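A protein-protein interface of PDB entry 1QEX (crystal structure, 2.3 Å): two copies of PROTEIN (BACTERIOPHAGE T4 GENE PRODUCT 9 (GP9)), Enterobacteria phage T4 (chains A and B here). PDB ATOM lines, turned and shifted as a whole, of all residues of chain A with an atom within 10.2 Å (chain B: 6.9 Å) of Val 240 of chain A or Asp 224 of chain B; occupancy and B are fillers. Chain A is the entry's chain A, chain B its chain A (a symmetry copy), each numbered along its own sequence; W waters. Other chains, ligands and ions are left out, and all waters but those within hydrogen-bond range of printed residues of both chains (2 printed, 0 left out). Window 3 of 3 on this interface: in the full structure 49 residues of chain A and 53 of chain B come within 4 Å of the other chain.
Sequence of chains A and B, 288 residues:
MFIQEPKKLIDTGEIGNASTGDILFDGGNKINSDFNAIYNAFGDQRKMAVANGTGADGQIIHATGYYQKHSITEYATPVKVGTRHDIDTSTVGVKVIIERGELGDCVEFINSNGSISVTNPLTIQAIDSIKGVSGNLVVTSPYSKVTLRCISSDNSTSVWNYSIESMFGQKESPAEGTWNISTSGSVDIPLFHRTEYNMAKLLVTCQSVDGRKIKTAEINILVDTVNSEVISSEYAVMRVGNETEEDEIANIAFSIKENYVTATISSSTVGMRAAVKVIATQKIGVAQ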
ATOM      1  N   THR A 205      26.815  -3.607  22.548  1.00  0.00           N
ATOM      2  CA  THR A 205      26.122  -3.818  21.288  1.00  0.00           C
ATOM      3  C   THR A 205      25.668  -5.274  21.205  1.00  0.00           C
ATOM      4  O   THR A 205      26.492  -6.187  21.175  1.00  0.00           O
ATOM      5  CB  THR A 205      27.043  -3.515  20.098  1.00  0.00           C
ATOM      6  OG1 THR A 205      27.381  -2.120  20.099  1.00  0.00           O
ATOM      7  CG2 THR A 205      26.354  -3.881  18.786  1.00  0.00           C
ATOM      8  N   CYS A 206      24.352  -5.469  21.183  1.00  0.00           N
ATOM      9  CA  CYS A 206      23.748  -6.792  21.112  1.00  0.00           C
ATOM     10  C   CYS A 206      23.151  -6.996  19.725  1.00  0.00           C
ATOM     11  O   CYS A 206      22.449  -6.124  19.208  1.00  0.00           O
ATOM     12  CB  CYS A 206      22.664  -6.923  22.177  1.00  0.00           C
ATOM     13  SG  CYS A 206      23.301  -6.700  23.859  1.00  0.00           S
ATOM     14  N   GLN A 207      23.435  -8.151  19.131  1.00  0.00           N
ATOM     15  CA  GLN A 207      22.958  -8.453  17.790  1.00  0.00           C
ATOM     16  C   GLN A 207      22.567  -9.918  17.657  1.00  0.00           C
ATOM     17  O   GLN A 207      23.258 -10.799  18.164  1.00  0.00           O
ATOM     18  CB  GLN A 207      24.062  -8.135  16.785  1.00  0.00           C
ATOM     19  CG  GLN A 207      23.668  -8.247  15.328  1.00  0.00           C
ATOM     20  CD  GLN A 207      24.876  -8.275  14.414  1.00  0.00           C
ATOM     21  OE1 GLN A 207      24.907  -7.603  13.386  1.00  0.00           O
ATOM     22  NE2 GLN A 207      25.879  -9.066  14.786  1.00  0.00           N
ATOM     23  N   SER A 208      21.463 -10.172  16.967  1.00  0.00           N
ATOM     24  CA  SER A 208      20.986 -11.537  16.756  1.00  0.00           C
ATOM     25  C   SER A 208      21.879 -12.231  15.733  1.00  0.00           C
ATOM     26  O   SER A 208      22.436 -11.581  14.851  1.00  0.00           O
ATOM     27  CB  SER A 208      19.550 -11.513  16.245  1.00  0.00           C
ATOM     28  OG  SER A 208      19.471 -10.785  15.030  1.00  0.00           O
ATOM     29  N   ASP A 210      21.286 -13.639  13.218  1.00  0.00           N
ATOM     30  CA  ASP A 210      20.835 -13.352  11.860  1.00  0.00           C
ATOM     31  C   ASP A 210      21.082 -11.900  11.454  1.00  0.00           C
ATOM     32  O   ASP A 210      21.217 -11.596  10.270  1.00  0.00           O
ATOM     33  CB  ASP A 210      19.350 -13.679  11.731  1.00  0.00           C
ATOM     34  CG  ASP A 210      18.515 -12.982  12.779  1.00  0.00           C
ATOM     35  OD1 ASP A 210      18.556 -11.734  12.827  1.00  0.00           O
ATOM     36  OD2 ASP A 210      17.826 -13.679  13.555  1.00  0.00           O
ATOM     37  N   GLY A 211      21.117 -11.005  12.435  1.00  0.00           N
ATOM     38  CA  GLY A 211      21.372  -9.605  12.148  1.00  0.00           C
ATOM     39  C   GLY A 211      20.168  -8.702  11.958  1.00  0.00           C
ATOM     40  O   GLY A 211      20.322  -7.545  11.560  1.00  0.00           O
ATOM     41  N   ARG A 212      18.973  -9.208  12.241  1.00  0.00           N
ATOM     42  CA  ARG A 212      17.763  -8.407  12.079  1.00  0.00           C
ATOM     43  C   ARG A 212      17.461  -7.603  13.337  1.00  0.00           C
ATOM     44  O   ARG A 212      16.783  -6.583  13.281  1.00  0.00           O
ATOM     45  CB  ARG A 212      16.572  -9.310  11.735  1.00  0.00           C
ATOM     46  CG  ARG A 212      16.206 -10.300  12.833  1.00  0.00           C
ATOM     47  CD  ARG A 212      15.432 -11.495  12.282  1.00  0.00           C
ATOM     48  NE  ARG A 212      15.179 -12.508  13.309  1.00  0.00           N
ATOM     49  CZ  ARG A 212      14.360 -12.340  14.345  1.00  0.00           C
ATOM     50  NH1 ARG A 212      13.702 -11.197  14.501  1.00  0.00           N
ATOM     51  NH2 ARG A 212      14.196 -13.319  15.228  1.00  0.00           N
ATOM     52  N   LYS A 213      17.956  -8.072  14.476  1.00  0.00           N
ATOM     53  CA  LYS A 213      17.742  -7.369  15.736  1.00  0.00           C
ATOM     54  C   LYS A 213      19.081  -6.899  16.283  1.00  0.00           C
ATOM     55  O   LYS A 213      20.018  -7.690  16.438  1.00  0.00           O
ATOM     56  CB  LYS A 213      17.055  -8.282  16.758  1.00  0.00           C
ATOM     57  CG  LYS A 213      15.530  -8.293  16.692  1.00  0.00           C
ATOM     58  CD  LYS A 213      14.957  -9.250  17.732  1.00  0.00           C
ATOM     59  CE  LYS A 213      13.437  -9.165  17.836  1.00  0.00           C
ATOM     60  NZ  LYS A 213      12.954  -7.979  18.613  1.00  0.00           N
ATOM     61  N   ILE A 214      19.178  -5.610  16.569  1.00  0.00           N
ATOM     62  CA  ILE A 214      20.418  -5.073  17.105  1.00  0.00           C
ATOM     63  C   ILE A 214      20.194  -3.820  17.933  1.00  0.00           C
ATOM     64  O   ILE A 214      19.372  -2.971  17.590  1.00  0.00           O
ATOM     65  CB  ILE A 214      21.431  -4.757  15.979  1.00  0.00           C
ATOM     66  CG1 ILE A 214      22.717  -4.182  16.581  1.00  0.00           C
ATOM     67  CG2 ILE A 214      20.826  -3.776  14.989  1.00  0.00           C
ATOM     68  CD1 ILE A 214      23.862  -4.059  15.592  1.00  0.00           C
ATOM     69  N   LYS A 215      20.919  -3.735  19.044  1.00  0.00           N
ATOM     70  CA  LYS A 215      20.847  -2.587  19.937  1.00  0.00           C
ATOM     71  C   LYS A 215      22.239  -2.230  20.457  1.00  0.00           C
ATOM     72  O   LYS A 215      23.068  -3.108  20.705  1.00  0.00           O
ATOM     73  CB  LYS A 215      19.951  -2.875  21.146  1.00  0.00           C
ATOM     74  CG  LYS A 215      20.074  -1.791  22.204  1.00  0.00           C
ATOM     75  CD  LYS A 215      19.555  -2.185  23.574  1.00  0.00           C
ATOM     76  CE  LYS A 215      19.924  -1.107  24.596  1.00  0.00           C
ATOM     77  NZ  LYS A 215      19.293  -1.296  25.937  1.00  0.00           N
ATOM     78  N   THR A 216      22.495  -0.935  20.602  1.00  0.00           N
ATOM     79  CA  THR A 216      23.760  -0.462  21.148  1.00  0.00           C
ATOM     80  C   THR A 216      23.396   0.610  22.153  1.00  0.00           C
ATOM     81  O   THR A 216      22.382   1.294  22.015  1.00  0.00           O
ATOM     82  CB  THR A 216      24.696   0.168  20.094  1.00  0.00           C
ATOM     83  OG1 THR A 216      24.099   1.357  19.571  1.00  0.00           O
ATOM     84  CG2 THR A 216      24.952  -0.794  18.969  1.00  0.00           C
ATOM     85  N   VAL A 237      20.814   5.226  23.258  1.00  0.00           N
ATOM     86  CA  VAL A 237      20.333   3.920  22.873  1.00  0.00           C
ATOM     87  C   VAL A 237      19.845   3.933  21.429  1.00  0.00           C
ATOM     88  O   VAL A 237      19.138   4.847  21.025  1.00  0.00           O
ATOM     89  CB  VAL A 237      19.181   3.494  23.806  1.00  0.00           C
ATOM     90  CG1 VAL A 237      18.514   2.232  23.281  1.00  0.00           C
ATOM     91  CG2 VAL A 237      19.729   3.267  25.215  1.00  0.00           C
ATOM     92  N   MET A 238      20.253   2.938  20.647  1.00  0.00           N
ATOM     93  CA  MET A 238      19.802   2.817  19.256  1.00  0.00           C
ATOM     94  C   MET A 238      19.429   1.362  18.943  1.00  0.00           C
ATOM     95  O   MET A 238      20.177   0.441  19.263  1.00  0.00           O
ATOM     96  CB  MET A 238      20.872   3.327  18.274  1.00  0.00           C
ATOM     97  CG  MET A 238      21.031   4.851  18.290  1.00  0.00           C
ATOM     98  SD  MET A 238      22.406   5.489  17.285  1.00  0.00           S
ATOM     99  CE  MET A 238      23.806   5.039  18.335  1.00  0.00           C
ATOM    100  N   ARG A 239      18.263   1.171  18.325  1.00  0.00           N
ATOM    101  CA  ARG A 239      17.752  -0.157  17.973  1.00  0.00           C
ATOM    102  C   ARG A 239      17.326  -0.222  16.497  1.00  0.00           C
ATOM    103  O   ARG A 239      16.944   0.798  15.916  1.00  0.00           O
ATOM    104  CB  ARG A 239      16.550  -0.487  18.860  1.00  0.00           C
ATOM    105  CG  ARG A 239      16.695   0.005  20.288  1.00  0.00           C
ATOM    106  CD  ARG A 239      15.619  -0.552  21.207  1.00  0.00           C
ATOM    107  NE  ARG A 239      14.277  -0.041  20.929  1.00  0.00           N
ATOM    108  CZ  ARG A 239      13.906   1.227  21.087  1.00  0.00           C
ATOM    109  NH1 ARG A 239      14.776   2.129  21.516  1.00  0.00           N
ATOM    110  NH2 ARG A 239      12.656   1.589  20.835  1.00  0.00           N
ATOM    111  N   VAL A 240      17.374  -1.410  15.898  1.00  0.00           N
ATOM    112  CA  VAL A 240      16.982  -1.566  14.500  1.00  0.00           C
ATOM    113  C   VAL A 240      15.759  -2.460  14.240  1.00  0.00           C
ATOM    114  O   VAL A 240      14.715  -1.976  13.787  1.00  0.00           O
ATOM    115  CB  VAL A 240      18.178  -2.064  13.636  1.00  0.00           C
ATOM    116  CG1 VAL A 240      17.677  -2.777  12.375  1.00  0.00           C
ATOM    117  CG2 VAL A 240      19.037  -0.869  13.225  1.00  0.00           C
ATOM    118  N   GLY A 241      15.881  -3.756  14.509  1.00  0.00           N
ATOM    119  CA  GLY A 241      14.761  -4.652  14.269  1.00  0.00           C
ATOM    120  C   GLY A 241      13.875  -4.823  15.484  1.00  0.00           C
ATOM    121  O   GLY A 241      13.497  -5.936  15.834  1.00  0.00           O
ATOM    122  N   ASN A 242      13.545  -3.708  16.125  1.00  0.00           N
ATOM    123  CA  ASN A 242      12.712  -3.709  17.318  1.00  0.00           C
ATOM    124  C   ASN A 242      11.227  -3.772  16.989  1.00  0.00           C
ATOM    125  O   ASN A 242      10.641  -2.790  16.540  1.00  0.00           O
ATOM    126  CB  ASN A 242      13.001  -2.457  18.138  1.00  0.00           C
ATOM    127  CG  ASN A 242      12.946  -1.198  17.305  1.00  0.00           C
ATOM    128  OD1 ASN A 242      12.065  -0.362  17.482  1.00  0.00           O
ATOM    129  ND2 ASN A 242      13.893  -1.055  16.387  1.00  0.00           N
ATOM    130  N   GLU A 243      10.620  -4.926  17.235  1.00  0.00           N
ATOM    131  CA  GLU A 243       9.204  -5.120  16.955  1.00  0.00           C
ATOM    132  C   GLU A 243       8.266  -4.113  17.627  1.00  0.00           C
ATOM    133  O   GLU A 243       7.118  -3.971  17.216  1.00  0.00           O
ATOM    134  CB  GLU A 243       8.806  -6.547  17.325  1.00  0.00           C
ATOM    135  CG  GLU A 243       9.476  -7.590  16.443  1.00  0.00           C
ATOM    136  CD  GLU A 243       9.209  -9.008  16.905  1.00  0.00           C
ATOM    137  OE1 GLU A 243       8.025  -9.346  17.142  1.00  0.00           O
ATOM    138  OE2 GLU A 243      10.184  -9.787  17.024  1.00  0.00           O
ATOM    139  N   THR A 244       8.752  -3.407  18.642  1.00  0.00           N
ATOM    140  CA  THR A 244       7.931  -2.416  19.338  1.00  0.00           C
ATOM    141  C   THR A 244       8.801  -1.316  19.945  1.00  0.00           C
ATOM    142  O   THR A 244       9.967  -1.547  20.266  1.00  0.00           O
ATOM    143  CB  THR A 244       7.104  -3.065  20.472  1.00  0.00           C
ATOM    144  OG1 THR A 244       6.379  -4.189  19.960  1.00  0.00           O
ATOM    145  CG2 THR A 244       6.117  -2.062  21.045  1.00  0.00           C
ATOM    146  N   GLU A 245       8.236  -0.122  20.102  1.00  0.00           N
ATOM    147  CA  GLU A 245       8.982   0.999  20.671  1.00  0.00           C
ATOM    148  C   GLU A 245       8.984   0.964  22.200  1.00  0.00           C
ATOM    149  O   GLU A 245       9.276   1.972  22.851  1.00  0.00           O
ATOM    150  CB  GLU A 245       8.400   2.329  20.181  1.00  0.00           C
ATOM    151  CG  GLU A 245       8.613   2.614  18.691  1.00  0.00           C
ATOM    152  CD  GLU A 245       8.082   1.503  17.787  1.00  0.00           C
ATOM    153  OE1 GLU A 245       6.922   1.071  17.988  1.00  0.00           O
ATOM    154  OE2 GLU A 245       8.822   1.064  16.874  1.00  0.00           O
ATOM    155  N   GLU A 248      12.895  -3.240  24.739  1.00  0.00           N
ATOM    156  CA  GLU A 248      13.253  -4.000  23.549  1.00  0.00           C
ATOM    157  C   GLU A 248      14.686  -4.440  23.241  1.00  0.00           C
ATOM    158  O   GLU A 248      15.668  -3.742  23.510  1.00  0.00           O
ATOM    159  CB  GLU A 248      12.715  -3.255  22.325  1.00  0.00           C
ATOM    160  CG  GLU A 248      12.629  -4.109  21.082  1.00  0.00           C
ATOM    161  CD  GLU A 248      11.658  -5.264  21.251  1.00  0.00           C
ATOM    162  OE1 GLU A 248      10.488  -5.001  21.594  1.00  0.00           O
ATOM    163  OE2 GLU A 248      12.065  -6.426  21.038  1.00  0.00           O
ATOM    164  N   ILE A 249      14.744  -5.619  22.623  1.00  0.00           N
ATOM    165  CA  ILE A 249      15.951  -6.280  22.159  1.00  0.00           C
ATOM    166  C   ILE A 249      16.892  -6.794  23.236  1.00  0.00           C
ATOM    167  O   ILE A 249      17.299  -7.955  23.190  1.00  0.00           O
ATOM    168  CB  ILE A 249      16.713  -5.374  21.158  1.00  0.00           C
ATOM    169  CG1 ILE A 249      15.761  -4.961  20.025  1.00  0.00           C
ATOM    170  CG2 ILE A 249      17.900  -6.118  20.569  1.00  0.00           C
ATOM    171  CD1 ILE A 249      16.383  -4.074  18.964  1.00  0.00           C
ATOM    172  N   ALA A 250      17.251  -5.953  24.199  1.00  0.00           N
ATOM    173  CA  ALA A 250      18.149  -6.407  25.252  1.00  0.00           C
ATOM    174  C   ALA A 250      18.238  -5.437  26.409  1.00  0.00           C
ATOM    175  O   ALA A 250      18.285  -4.216  26.218  1.00  0.00           O
ATOM    176  CB  ALA A 250      19.542  -6.662  24.684  1.00  0.00           C
ATOM    177  N   MET A 272      21.116 -14.415  20.828  1.00  0.00           N
ATOM    178  CA  MET A 272      21.694 -13.075  20.856  1.00  0.00           C
ATOM    179  C   MET A 272      23.144 -13.058  21.318  1.00  0.00           C
ATOM    180  O   MET A 272      23.523 -13.796  22.226  1.00  0.00           O
ATOM    181  CB  MET A 272      20.881 -12.172  21.781  1.00  0.00           C
ATOM    182  CG  MET A 272      19.555 -11.711  21.212  1.00  0.00           C
ATOM    183  SD  MET A 272      19.766 -10.479  19.915  1.00  0.00           S
ATOM    184  CE  MET A 272      20.180  -9.051  20.877  1.00  0.00           C
ATOM    185  N   ARG B 194      31.558  -0.279   5.711  1.00  0.00           N
ATOM    186  CA  ARG B 194      30.385  -0.740   6.433  1.00  0.00           C
ATOM    187  C   ARG B 194      30.572  -2.020   7.256  1.00  0.00           C
ATOM    188  O   ARG B 194      29.819  -2.260   8.190  1.00  0.00           O
ATOM    189  CB  ARG B 194      29.239  -0.953   5.454  1.00  0.00           C
ATOM    190  CG  ARG B 194      29.541  -2.009   4.420  1.00  0.00           C
ATOM    191  CD  ARG B 194      28.284  -2.724   4.020  1.00  0.00           C
ATOM    192  NE  ARG B 194      27.552  -2.065   2.951  1.00  0.00           N
ATOM    193  CZ  ARG B 194      26.233  -2.104   2.824  1.00  0.00           C
ATOM    194  NH1 ARG B 194      25.495  -2.768   3.706  1.00  0.00           N
ATOM    195  NH2 ARG B 194      25.648  -1.464   1.827  1.00  0.00           N
ATOM    196  N   ASN B 198      30.266  -1.994  14.153  1.00  0.00           N
ATOM    197  CA  ASN B 198      28.820  -1.964  14.319  1.00  0.00           C
ATOM    198  C   ASN B 198      28.394  -0.601  14.861  1.00  0.00           C
ATOM    199  O   ASN B 198      27.288  -0.122  14.585  1.00  0.00           O
ATOM    200  CB  ASN B 198      28.354  -3.049  15.292  1.00  0.00           C
ATOM    201  CG  ASN B 198      28.727  -4.446  14.830  1.00  0.00           C
ATOM    202  OD1 ASN B 198      29.803  -4.950  15.147  1.00  0.00           O
ATOM    203  ND2 ASN B 198      27.839  -5.074  14.063  1.00  0.00           N
ATOM    204  N   LEU B 222      25.059   3.848  14.800  1.00  0.00           N
ATOM    205  CA  LEU B 222      24.866   2.410  14.706  1.00  0.00           C
ATOM    206  C   LEU B 222      24.745   2.017  13.245  1.00  0.00           C
ATOM    207  O   LEU B 222      23.943   2.587  12.506  1.00  0.00           O
ATOM    208  CB  LEU B 222      23.603   1.992  15.458  1.00  0.00           C
ATOM    209  CG  LEU B 222      23.178   0.543  15.209  1.00  0.00           C
ATOM    210  CD1 LEU B 222      24.264  -0.409  15.680  1.00  0.00           C
ATOM    211  CD2 LEU B 222      21.854   0.279  15.917  1.00  0.00           C
ATOM    212  N   VAL B 223      25.538   1.042  12.825  1.00  0.00           N
ATOM    213  CA  VAL B 223      25.498   0.606  11.445  1.00  0.00           C
ATOM    214  C   VAL B 223      24.428  -0.456  11.225  1.00  0.00           C
ATOM    215  O   VAL B 223      24.486  -1.538  11.803  1.00  0.00           O
ATOM    216  CB  VAL B 223      26.856   0.042  10.999  1.00  0.00           C
ATOM    217  CG1 VAL B 223      26.781  -0.393   9.532  1.00  0.00           C
ATOM    218  CG2 VAL B 223      27.940   1.089  11.197  1.00  0.00           C
ATOM    219  N   ASP B 224      23.439  -0.125  10.403  1.00  0.00           N
ATOM    220  CA  ASP B 224      22.365  -1.049  10.076  1.00  0.00           C
ATOM    221  C   ASP B 224      22.749  -1.648   8.724  1.00  0.00           C
ATOM    222  O   ASP B 224      22.369  -1.120   7.678  1.00  0.00           O
ATOM    223  CB  ASP B 224      21.036  -0.297   9.946  1.00  0.00           C
ATOM    224  CG  ASP B 224      19.874  -1.223   9.615  1.00  0.00           C
ATOM    225  OD1 ASP B 224      20.121  -2.334   9.111  1.00  0.00           O
ATOM    226  OD2 ASP B 224      18.717  -0.833   9.849  1.00  0.00           O
ATOM    227  N   THR B 225      23.516  -2.734   8.745  1.00  0.00           N
ATOM    228  CA  THR B 225      23.952  -3.350   7.502  1.00  0.00           C
ATOM    229  C   THR B 225      22.795  -3.899   6.667  1.00  0.00           C
ATOM    230  O   THR B 225      22.816  -3.812   5.444  1.00  0.00           O
ATOM    231  CB  THR B 225      24.972  -4.495   7.753  1.00  0.00           C
ATOM    232  OG1 THR B 225      24.350  -5.545   8.500  1.00  0.00           O
ATOM    233  CG2 THR B 225      26.173  -3.976   8.509  1.00  0.00           C
ATOM    234  N   VAL B 226      21.782  -4.441   7.330  1.00  0.00           N
ATOM    235  CA  VAL B 226      20.639  -5.012   6.633  1.00  0.00           C
ATOM    236  C   VAL B 226      19.874  -4.011   5.764  1.00  0.00           C
ATOM    237  O   VAL B 226      19.486  -4.336   4.650  1.00  0.00           O
ATOM    238  CB  VAL B 226      19.663  -5.676   7.631  1.00  0.00           C
ATOM    239  CG1 VAL B 226      18.435  -6.203   6.902  1.00  0.00           C
ATOM    240  CG2 VAL B 226      20.372  -6.815   8.355  1.00  0.00           C
ATOM    241  N   ASN B 227      19.659  -2.803   6.271  1.00  0.00           N
ATOM    242  CA  ASN B 227      18.938  -1.781   5.515  1.00  0.00           C
ATOM    243  C   ASN B 227      19.909  -0.782   4.879  1.00  0.00           C
ATOM    244  O   ASN B 227      19.494   0.234   4.320  1.00  0.00           O
ATOM    245  CB  ASN B 227      17.974  -1.030   6.434  1.00  0.00           C
ATOM    246  CG  ASN B 227      16.984  -1.947   7.118  1.00  0.00           C
ATOM    247  OD1 ASN B 227      16.132  -1.494   7.889  1.00  0.00           O
ATOM    248  ND2 ASN B 227      17.088  -3.244   6.844  1.00  0.00           N
ATOM    249  N   SER B 228      21.202  -1.078   4.979  1.00  0.00           N
ATOM    250  CA  SER B 228      22.234  -0.203   4.432  1.00  0.00           C
ATOM    251  C   SER B 228      22.086   1.240   4.908  1.00  0.00           C
ATOM    252  O   SER B 228      22.200   2.173   4.113  1.00  0.00           O
ATOM    253  CB  SER B 228      22.215  -0.242   2.904  1.00  0.00           C
ATOM    254  OG  SER B 228      22.691  -1.489   2.428  1.00  0.00           O
ATOM    255  N   GLU B 229      21.834   1.413   6.205  1.00  0.00           N
ATOM    256  CA  GLU B 229      21.682   2.740   6.797  1.00  0.00           C
ATOM    257  C   GLU B 229      22.515   2.882   8.068  1.00  0.00           C
ATOM    258  O   GLU B 229      23.191   1.952   8.498  1.00  0.00           O
ATOM    259  CB  GLU B 229      20.222   3.008   7.149  1.00  0.00           C
ATOM    260  CG  GLU B 229      19.257   2.772   6.021  1.00  0.00           C
ATOM    261  CD  GLU B 229      17.865   3.272   6.335  1.00  0.00           C
ATOM    262  OE1 GLU B 229      17.299   2.883   7.377  1.00  0.00           O
ATOM    263  OE2 GLU B 229      17.333   4.062   5.535  1.00  0.00           O
ATOM    264  N   VAL B 230      22.452   4.061   8.671  1.00  0.00           N
ATOM    265  CA  VAL B 230      23.179   4.314   9.903  1.00  0.00           C
ATOM    266  C   VAL B 230      22.354   5.199  10.817  1.00  0.00           C
ATOM    267  O   VAL B 230      21.990   6.301  10.434  1.00  0.00           O
ATOM    268  CB  VAL B 230      24.518   5.012   9.630  1.00  0.00           C
ATOM    269  CG1 VAL B 230      24.282   6.255   8.824  1.00  0.00           C
ATOM    270  CG2 VAL B 230      25.207   5.367  10.945  1.00  0.00           C
ATOM    271  N   ILE B 231      22.033   4.689  12.008  1.00  0.00           N
ATOM    272  CA  ILE B 231      21.275   5.457  12.997  1.00  0.00           C
ATOM    273  C   ILE B 231      22.283   6.294  13.772  1.00  0.00           C
ATOM    274  O   ILE B 231      23.410   5.860  13.993  1.00  0.00           O
ATOM    275  CB  ILE B 231      20.533   4.553  14.029  1.00  0.00           C
ATOM    276  CG1 ILE B 231      19.560   3.608  13.322  1.00  0.00           C
ATOM    277  CG2 ILE B 231      19.765   5.416  15.018  1.00  0.00           C
ATOM    278  CD1 ILE B 231      20.218   2.364  12.798  1.00  0.00           C
ATOM    279  N   ILE B 256      25.334   5.399   4.387  1.00  0.00           N
ATOM    280  CA  ILE B 256      26.341   4.577   3.749  1.00  0.00           C
ATOM    281  C   ILE B 256      26.426   5.042   2.292  1.00  0.00           C
ATOM    282  O   ILE B 256      25.421   5.084   1.582  1.00  0.00           O
ATOM    283  CB  ILE B 256      25.982   3.080   3.772  1.00  0.00           C
ATOM    284  CG1 ILE B 256      25.944   2.562   5.210  1.00  0.00           C
ATOM    285  CG2 ILE B 256      27.016   2.300   2.986  1.00  0.00           C
ATOM    286  CD1 ILE B 256      25.798   1.036   5.295  1.00  0.00           C
HETATM  287  O   HOH W   1      27.975  -7.673  12.266  1.00  0.00           O
HETATM  288  O   HOH W   2      20.952  -4.586  10.466  1.00  0.00           O
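Asn 198 of chain B touches Gln 207 of chain A (ND2 to OE1, 3.9 Å).
Val 226 of chain B touches Gly 211 of chain A.
Ile 214 of chain A touches Leu 222 of chain B.
Leu 222 of chain B touches Thr 216 of chain A (CD1 to CG2, 3.4 Å).
Met 238 of chain A touches Leu 222 of chain B.
Val 240 of chain A touches Asp 224 of chain B.
CD1 of Ile 231 of chain B touches CG2 of Val 240 of chain A, 3.5 Å away.
The backbone NH (N) of Gly 211 of chain A sits at hydrogen-bond distance from the side-chain hydroxyl (OG) of Ser 208 of chain A (3.1 Å).
The backbone NH (N) of Val 226 of chain B sits at hydrogen-bond distance from the side-chain carboxylate (OD1) of Asp 224 of chain B (3.2 Å).
The backbone NH (N) of Asp 224 of chain B lies within hydrogen-bond range of the backbone carbonyl oxygen (O) of Glu 229 of chain B (2.8 Å).
O of Asn 198 of chain B sits at hydrogen-bond distance from N of Val 223 of chain B (2.7 Å).
ND2 of Asn 242 of chain A lies within hydrogen-bond range of O of Val 240 of chain A, at 2.9 Å.
The backbone NH (N) of Leu 222 of chain B sits at hydrogen-bond distance from the backbone carbonyl oxygen (O) of Ile 231 of chain B, 2.7 Å away.
Water W2 lies within hydrogen-bond range of the side-chain carboxylate (OD1) of Asp 224 of chain B, the backbone carbonyl oxygen (O) of Gly 211 of chain A and the backbone NH (N) of Val 226 of chain B.
Water W1 bridges ND2 of Asn 198 of chain B (3.2 Å) and OE1 of Gln 207 of chain A (3.3 Å).
No position is printed for both chains.
Of the 8 pairs that touch across the chains among the printed residues, none has its exchanged pair printed and touching as well.
The side-chain sulfur of Met 238 of chain A sits close to the backbone carbonyl oxygen of Ile 231 of chain B.
Of chain A, only Val 240 (3.4 Å) comes within 4 Å of Asp 224 of chain B.
Of the printed residues of chain A, Leu 222 of chain B touches Ile 214, Thr 216 and Met 238.
No residue of chain A comes within 4 Å of Val 223 of chain B.
No residue of chain A comes within 4 Å of Thr 225 of chain B.
No residue of chain A comes within 4 Å of Asn 227 of chain B.
No residue of chain A comes within 4 Å of Ser 228 of chain B.
Of the printed residues of chain B, Thr 216 of chain A touches Leu 222 (3.4 Å).
Of the printed residues of chain B, Ile 214 of chain A touches Leu 222.
Thr 244 of chain A touches none of the printed residues of chain B.
Lys 213 of chain A touches none of the printed residues of chain B.
The nearest printed residue of chain B that does not touch Ile 214 of chain A is Asn 198 of chain B (4.4 Å).
Printed residues of chain B that touch a printed residue of chain A: Asn 198, Leu 222, Asp 224, Val 226 and Ile 231.
Hydrophobic or aromatic side chains of chain B that line the printed part of chain A: Leu 222, Val 226 and Ile 231.
Among the printed residues, 8 pairs touch across the chains.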
